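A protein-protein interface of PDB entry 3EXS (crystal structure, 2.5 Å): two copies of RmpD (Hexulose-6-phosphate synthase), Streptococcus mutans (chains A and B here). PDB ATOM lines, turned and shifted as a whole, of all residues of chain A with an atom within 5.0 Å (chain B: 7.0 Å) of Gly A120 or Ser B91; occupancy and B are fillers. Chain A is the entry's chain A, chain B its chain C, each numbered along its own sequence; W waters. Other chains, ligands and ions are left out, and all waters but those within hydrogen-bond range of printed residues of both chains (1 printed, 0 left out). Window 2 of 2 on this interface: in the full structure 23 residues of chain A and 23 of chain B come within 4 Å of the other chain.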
ATOM      1  N   ILE A  89       2.623 -28.029   2.491  1.00  0.00           N
ATOM      2  CA  ILE A  89       3.656 -28.143   1.430  1.00  0.00           C
ATOM      3  C   ILE A  89       3.513 -29.479   0.708  1.00  0.00           C
ATOM      4  O   ILE A  89       3.189 -30.493   1.322  1.00  0.00           O
ATOM      5  CB  ILE A  89       5.084 -27.984   2.000  1.00  0.00           C
ATOM      6  CG1 ILE A  89       6.106 -27.804   0.877  1.00  0.00           C
ATOM      7  CG2 ILE A  89       5.440 -29.140   2.903  1.00  0.00           C
ATOM      8  CD1 ILE A  89       6.227 -26.377   0.362  1.00  0.00           C
ATOM      9  N   SER A  91       5.318 -31.702  -0.177  1.00  0.00           N
ATOM     10  CA  SER A  91       6.188 -32.804   0.299  1.00  0.00           C
ATOM     11  C   SER A  91       5.728 -33.431   1.616  1.00  0.00           C
ATOM     12  O   SER A  91       6.256 -34.472   2.047  1.00  0.00           O
ATOM     13  CB  SER A  91       7.669 -32.394   0.353  1.00  0.00           C
ATOM     14  OG  SER A  91       7.815 -31.028   0.675  1.00  0.00           O
ATOM     15  N   LEU A 118       2.770 -25.929  -4.065  1.00  0.00           N
ATOM     16  CA  LEU A 118       3.585 -26.645  -5.025  1.00  0.00           C
ATOM     17  C   LEU A 118       4.935 -26.000  -5.077  1.00  0.00           C
ATOM     18  O   LEU A 118       5.097 -24.878  -5.564  1.00  0.00           O
ATOM     19  CB  LEU A 118       2.922 -26.609  -6.394  1.00  0.00           C
ATOM     20  CG  LEU A 118       1.524 -27.226  -6.430  1.00  0.00           C
ATOM     21  CD1 LEU A 118       0.833 -26.936  -7.726  1.00  0.00           C
ATOM     22  CD2 LEU A 118       1.615 -28.718  -6.205  1.00  0.00           C
ATOM     23  N   TYR A 119       5.909 -26.711  -4.534  1.00  0.00           N
ATOM     24  CA  TYR A 119       7.296 -26.311  -4.617  1.00  0.00           C
ATOM     25  C   TYR A 119       8.135 -27.512  -5.060  1.00  0.00           C
ATOM     26  O   TYR A 119       7.770 -28.647  -4.763  1.00  0.00           O
ATOM     27  CB  TYR A 119       7.751 -25.822  -3.249  1.00  0.00           C
ATOM     28  CG  TYR A 119       7.427 -24.372  -2.952  1.00  0.00           C
ATOM     29  CD1 TYR A 119       8.354 -23.366  -3.201  1.00  0.00           C
ATOM     30  CD2 TYR A 119       6.200 -24.012  -2.395  1.00  0.00           C
ATOM     31  CE1 TYR A 119       8.046 -22.023  -2.902  1.00  0.00           C
ATOM     32  CE2 TYR A 119       5.882 -22.684  -2.111  1.00  0.00           C
ATOM     33  CZ  TYR A 119       6.798 -21.699  -2.366  1.00  0.00           C
ATOM     34  OH  TYR A 119       6.478 -20.401  -2.074  1.00  0.00           O
ATOM     35  N   GLY A 120       9.249 -27.272  -5.758  1.00  0.00           N
ATOM     36  CA  GLY A 120      10.136 -28.363  -6.206  1.00  0.00           C
ATOM     37  C   GLY A 120       9.467 -29.351  -7.163  1.00  0.00           C
ATOM     38  O   GLY A 120       8.490 -29.019  -7.841  1.00  0.00           O
ATOM     39  N   ASP A 121       9.974 -30.580  -7.190  1.00  0.00           N
ATOM     40  CA  ASP A 121       9.555 -31.596  -8.172  1.00  0.00           C
ATOM     41  C   ASP A 121       8.423 -32.475  -7.666  1.00  0.00           C
ATOM     42  O   ASP A 121       8.657 -33.584  -7.187  1.00  0.00           O
ATOM     43  CB  ASP A 121      10.743 -32.497  -8.567  1.00  0.00           C
ATOM     44  CG  ASP A 121      11.942 -31.708  -9.077  1.00  0.00           C
ATOM     45  OD1 ASP A 121      11.729 -30.695  -9.780  1.00  0.00           O
ATOM     46  OD2 ASP A 121      13.096 -32.111  -8.780  1.00  0.00           O
ATOM     47  N   TRP A 122       7.200 -31.987  -7.778  1.00  0.00           N
ATOM     48  CA  TRP A 122       6.004 -32.776  -7.435  1.00  0.00           C
ATOM     49  C   TRP A 122       5.476 -33.538  -8.678  1.00  0.00           C
ATOM     50  O   TRP A 122       5.798 -33.192  -9.811  1.00  0.00           O
ATOM     51  CB  TRP A 122       4.916 -31.838  -6.870  1.00  0.00           C
ATOM     52  CG  TRP A 122       4.609 -30.673  -7.812  1.00  0.00           C
ATOM     53  CD1 TRP A 122       5.253 -29.473  -7.858  1.00  0.00           C
ATOM     54  CD2 TRP A 122       3.624 -30.642  -8.850  1.00  0.00           C
ATOM     55  NE1 TRP A 122       4.729 -28.692  -8.856  1.00  0.00           N
ATOM     56  CE2 TRP A 122       3.724 -29.385  -9.481  1.00  0.00           C
ATOM     57  CE3 TRP A 122       2.661 -31.555  -9.305  1.00  0.00           C
ATOM     58  CZ2 TRP A 122       2.892 -29.005 -10.554  1.00  0.00           C
ATOM     59  CZ3 TRP A 122       1.830 -31.181 -10.373  1.00  0.00           C
ATOM     60  CH2 TRP A 122       1.954 -29.911 -10.980  1.00  0.00           C
ATOM     61  N   CYS B  67      11.726 -23.728   6.136  1.00  0.00           N
ATOM     62  CA  CYS B  67      11.603 -22.684   5.141  1.00  0.00           C
ATOM     63  C   CYS B  67      11.442 -23.241   3.730  1.00  0.00           C
ATOM     64  O   CYS B  67      12.265 -24.050   3.291  1.00  0.00           O
ATOM     65  CB  CYS B  67      12.873 -21.851   5.174  1.00  0.00           C
ATOM     66  SG  CYS B  67      12.769 -20.409   4.168  1.00  0.00           S
ATOM     67  N   ALA B  68      10.402 -22.813   3.026  1.00  0.00           N
ATOM     68  CA  ALA B  68      10.215 -23.202   1.625  1.00  0.00           C
ATOM     69  C   ALA B  68      10.486 -22.052   0.671  1.00  0.00           C
ATOM     70  O   ALA B  68      10.568 -22.269  -0.541  1.00  0.00           O
ATOM     71  CB  ALA B  68       8.815 -23.732   1.389  1.00  0.00           C
ATOM     72  N   CYS B  88      15.469 -25.614   6.250  1.00  0.00           N
ATOM     73  CA  CYS B  88      14.767 -25.424   4.983  1.00  0.00           C
ATOM     74  C   CYS B  88      14.193 -26.759   4.572  1.00  0.00           C
ATOM     75  O   CYS B  88      14.850 -27.788   4.717  1.00  0.00           O
ATOM     76  CB  CYS B  88      15.722 -24.978   3.901  1.00  0.00           C
ATOM     77  SG  CYS B  88      16.156 -23.228   3.984  1.00  0.00           S
ATOM     78  N   ILE B  89      12.959 -26.758   4.081  1.00  0.00           N
ATOM     79  CA  ILE B  89      12.344 -27.987   3.594  1.00  0.00           C
ATOM     80  C   ILE B  89      13.032 -28.333   2.273  1.00  0.00           C
ATOM     81  O   ILE B  89      13.418 -27.454   1.504  1.00  0.00           O
ATOM     82  CB  ILE B  89      10.797 -27.830   3.427  1.00  0.00           C
ATOM     83  CG1 ILE B  89      10.133 -29.162   3.102  1.00  0.00           C
ATOM     84  CG2 ILE B  89      10.429 -26.804   2.337  1.00  0.00           C
ATOM     85  CD1 ILE B  89       9.657 -29.880   4.279  1.00  0.00           C
ATOM     86  N   CYS B  90      13.197 -29.620   2.012  1.00  0.00           N
ATOM     87  CA  CYS B  90      13.942 -30.039   0.829  1.00  0.00           C
ATOM     88  C   CYS B  90      13.307 -29.568  -0.489  1.00  0.00           C
ATOM     89  O   CYS B  90      13.978 -29.525  -1.538  1.00  0.00           O
ATOM     90  CB  CYS B  90      14.159 -31.548   0.829  1.00  0.00           C
ATOM     91  SG  CYS B  90      12.663 -32.519   0.984  1.00  0.00           S
ATOM     92  N   SER B  91      12.027 -29.205  -0.450  1.00  0.00           N
ATOM     93  CA  SER B  91      11.405 -28.703  -1.670  1.00  0.00           C
ATOM     94  C   SER B  91      11.680 -27.217  -1.921  1.00  0.00           C
ATOM     95  O   SER B  91      11.279 -26.683  -2.948  1.00  0.00           O
ATOM     96  CB  SER B  91       9.917 -29.075  -1.787  1.00  0.00           C
ATOM     97  OG  SER B  91       9.309 -29.272  -0.533  1.00  0.00           O
ATOM     98  N   ALA B  92      12.402 -26.558  -1.019  1.00  0.00           N
ATOM     99  CA  ALA B  92      12.880 -25.216  -1.305  1.00  0.00           C
ATOM    100  C   ALA B  92      13.866 -25.240  -2.471  1.00  0.00           C
ATOM    101  O   ALA B  92      14.759 -26.101  -2.550  1.00  0.00           O
ATOM    102  CB  ALA B  92      13.527 -24.626  -0.095  1.00  0.00           C
ATOM    103  N   THR B  93      13.718 -24.294  -3.387  1.00  0.00           N
ATOM    104  CA  THR B  93      14.656 -24.179  -4.509  1.00  0.00           C
ATOM    105  C   THR B  93      16.057 -23.886  -3.995  1.00  0.00           C
ATOM    106  O   THR B  93      16.223 -23.382  -2.884  1.00  0.00           O
ATOM    107  CB  THR B  93      14.226 -23.080  -5.540  1.00  0.00           C
ATOM    108  OG1 THR B  93      14.396 -21.771  -4.965  1.00  0.00           O
ATOM    109  CG2 THR B  93      12.768 -23.277  -6.006  1.00  0.00           C
ATOM    110  N   ILE B  94      17.058 -24.215  -4.807  1.00  0.00           N
ATOM    111  CA  ILE B  94      18.440 -23.835  -4.532  1.00  0.00           C
ATOM    112  C   ILE B  94      18.602 -22.322  -4.254  1.00  0.00           C
ATOM    113  O   ILE B  94      19.231 -21.968  -3.249  1.00  0.00           O
ATOM    114  CB  ILE B  94      19.395 -24.313  -5.664  1.00  0.00           C
ATOM    115  CG1 ILE B  94      19.231 -25.811  -5.881  1.00  0.00           C
ATOM    116  CG2 ILE B  94      20.847 -23.938  -5.374  1.00  0.00           C
ATOM    117  CD1 ILE B  94      19.784 -26.640  -4.768  1.00  0.00           C
ATOM    118  N   MET B  97      17.594 -21.654  -0.789  1.00  0.00           N
ATOM    119  CA  MET B  97      18.532 -22.185   0.183  1.00  0.00           C
ATOM    120  C   MET B  97      19.777 -21.297   0.277  1.00  0.00           C
ATOM    121  O   MET B  97      20.342 -21.117   1.349  1.00  0.00           O
ATOM    122  CB  MET B  97      18.891 -23.633  -0.145  1.00  0.00           C
ATOM    123  CG  MET B  97      17.702 -24.569  -0.096  1.00  0.00           C
ATOM    124  SD  MET B  97      18.183 -26.295   0.142  1.00  0.00           S
ATOM    125  CE  MET B  97      16.594 -27.094   0.287  1.00  0.00           C
ATOM    126  N   VAL B 116      18.903 -29.308   5.884  1.00  0.00           N
ATOM    127  CA  VAL B 116      17.810 -29.679   4.971  1.00  0.00           C
ATOM    128  C   VAL B 116      16.886 -30.676   5.644  1.00  0.00           C
ATOM    129  O   VAL B 116      17.327 -31.736   6.102  1.00  0.00           O
ATOM    130  CB  VAL B 116      18.317 -30.242   3.622  1.00  0.00           C
ATOM    131  CG1 VAL B 116      17.159 -30.587   2.716  1.00  0.00           C
ATOM    132  CG2 VAL B 116      19.237 -29.236   2.939  1.00  0.00           C
ATOM    133  N   GLU B 117      15.606 -30.324   5.715  1.00  0.00           N
ATOM    134  CA  GLU B 117      14.586 -31.230   6.226  1.00  0.00           C
ATOM    135  C   GLU B 117      14.107 -32.199   5.125  1.00  0.00           C
ATOM    136  O   GLU B 117      13.583 -31.770   4.080  1.00  0.00           O
ATOM    137  CB  GLU B 117      13.416 -30.414   6.778  1.00  0.00           C
ATOM    138  CG  GLU B 117      13.561 -30.008   8.240  1.00  0.00           C
ATOM    139  CD  GLU B 117      13.344 -31.186   9.197  1.00  0.00           C
ATOM    140  OE1 GLU B 117      13.152 -32.312   8.707  1.00  0.00           O
ATOM    141  OE2 GLU B 117      13.372 -31.004  10.436  1.00  0.00           O
ATOM    142  N   TYR B 119      11.671 -34.618   3.554  1.00  0.00           N
ATOM    143  CA  TYR B 119      10.278 -35.044   3.518  1.00  0.00           C
ATOM    144  C   TYR B 119       9.909 -35.476   2.101  1.00  0.00           C
ATOM    145  O   TYR B 119      10.350 -34.866   1.130  1.00  0.00           O
ATOM    146  CB  TYR B 119       9.375 -33.895   3.968  1.00  0.00           C
ATOM    147  CG  TYR B 119       9.208 -33.863   5.465  1.00  0.00           C
ATOM    148  CD1 TYR B 119       8.227 -34.626   6.098  1.00  0.00           C
ATOM    149  CD2 TYR B 119      10.060 -33.093   6.263  1.00  0.00           C
ATOM    150  CE1 TYR B 119       8.087 -34.597   7.493  1.00  0.00           C
ATOM    151  CE2 TYR B 119       9.935 -33.074   7.655  1.00  0.00           C
ATOM    152  CZ  TYR B 119       8.947 -33.818   8.262  1.00  0.00           C
ATOM    153  OH  TYR B 119       8.830 -33.782   9.635  1.00  0.00           O
ATOM    154  N   GLN B 126      19.590 -33.943  -5.937  1.00  0.00           N
ATOM    155  CA  GLN B 126      19.192 -32.797  -5.117  1.00  0.00           C
ATOM    156  C   GLN B 126      20.184 -32.670  -3.958  1.00  0.00           C
ATOM    157  O   GLN B 126      20.763 -31.598  -3.748  1.00  0.00           O
ATOM    158  CB  GLN B 126      17.757 -32.926  -4.606  1.00  0.00           C
ATOM    159  CG  GLN B 126      16.669 -32.599  -5.638  1.00  0.00           C
ATOM    160  CD  GLN B 126      15.260 -33.094  -5.217  1.00  0.00           C
ATOM    161  OE1 GLN B 126      15.092 -33.760  -4.178  1.00  0.00           O
ATOM    162  NE2 GLN B 126      14.244 -32.773  -6.037  1.00  0.00           N
ATOM    163  N   TRP B 130      22.482 -29.352  -2.754  1.00  0.00           N
ATOM    164  CA  TRP B 130      22.568 -28.719  -1.468  1.00  0.00           C
ATOM    165  C   TRP B 130      24.038 -28.526  -1.095  1.00  0.00           C
ATOM    166  O   TRP B 130      24.458 -27.402  -0.757  1.00  0.00           O
ATOM    167  CB  TRP B 130      21.772 -29.502  -0.416  1.00  0.00           C
ATOM    168  CG  TRP B 130      20.341 -29.819  -0.871  1.00  0.00           C
ATOM    169  CD1 TRP B 130      19.540 -29.060  -1.707  1.00  0.00           C
ATOM    170  CD2 TRP B 130      19.574 -30.977  -0.532  1.00  0.00           C
ATOM    171  NE1 TRP B 130      18.334 -29.687  -1.907  1.00  0.00           N
ATOM    172  CE2 TRP B 130      18.321 -30.858  -1.190  1.00  0.00           C
ATOM    173  CE3 TRP B 130      19.816 -32.103   0.280  1.00  0.00           C
ATOM    174  CZ2 TRP B 130      17.317 -31.826  -1.069  1.00  0.00           C
ATOM    175  CZ3 TRP B 130      18.815 -33.072   0.407  1.00  0.00           C
ATOM    176  CH2 TRP B 130      17.579 -32.923  -0.273  1.00  0.00           C
HETATM  177  O   HOH W   1      12.000 -30.999  -4.786  1.00  0.00           O
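The side-chain amide nitrogen of Gln B126 sits at hydrogen-bond distance from the side-chain carboxylate of Asp A121 (3.0 Å).
The side-chain hydroxyl of Ser B91 is in hydrogen-bond range of the side-chain hydroxyl of Ser A91, 2.6 Å away.
The backbone carbonyl oxygen (O) of Tyr B119 sits at hydrogen-bond distance from the side-chain sulfur (SG) of Cys B90 (3.3 Å).
The backbone NH (N) of Ile B89 sits at hydrogen-bond distance from the backbone carbonyl oxygen (O) of Cys B67, at 2.9 Å.
Ile A89 touches Ala B68.
Ile A89 touches Ser B91.
Ile B89 touches Ser A91.
Tyr B119 touches Ser A91 (CB to O, 3.7 Å).
Tyr A119 touches Ala B68 (CE1 to O, 3.5 Å).
CB of Tyr A119 touches O of Ser B91 (3.6 Å).
N of Gly A120 touches O of Ser B91, at 3.5 Å.
Of the printed residues of chain B, Ser A91 touches Ile B89, Ser B91 and Tyr B119.
Of the printed residues of chain B, Tyr A119 touches Ala B68 (3.5 Å) and Ser B91 (3.6 Å).
Gly A120 touches one residue of chain B.
Cys B88 touches none of the printed residues of chain A.
Of chain A, only Ile A89, Ser A91, Tyr A119 and Gly A120 come within 4 Å of Ser B91.
Trp B130 touches none of the printed residues of chain A.
The nearest residue of chain B that does not touch Gly A120 is Thr B93 (5.3 Å).
The nearest printed residue of chain A that does not touch Ser B91 is Asp A121 (5.6 Å).
The nearest printed residue of chain B that does not touch Ser A91 is Cys B90 (5.0 Å).
Hydrophobic or aromatic side chains of chain B within 4 Å of the printed part of chain A: Ala B68, Ile B89 and Tyr B119.
Along chain B the printed residues that touch a printed residue of chain A span positions 68 to 126.
Hydrophobic or aromatic side chains of chain A within 4 Å of the printed part of chain B: Ile A89 and Tyr A119.
Among the printed residues, no Asp or Glu carboxylate lies within 4 Å of a Lys or Arg side-chain nitrogen of the other chain.
Ile A89 touches Ser B91, and with the chains exchanged Ser A91 touches Ile B89.
Ser B91 touches its own counterpart, Ser A91.
Ser A91 touches Tyr B119, and with the chains exchanged Tyr A119 touches Ser B91.
Positions printed for both chains: 89, 91 and 119.
Water W1 bridges the side-chain amide nitrogen (NE2) of Gln B126 (3.1 Å) and the backbone NH (N) of Asp A121 (3.2 Å).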
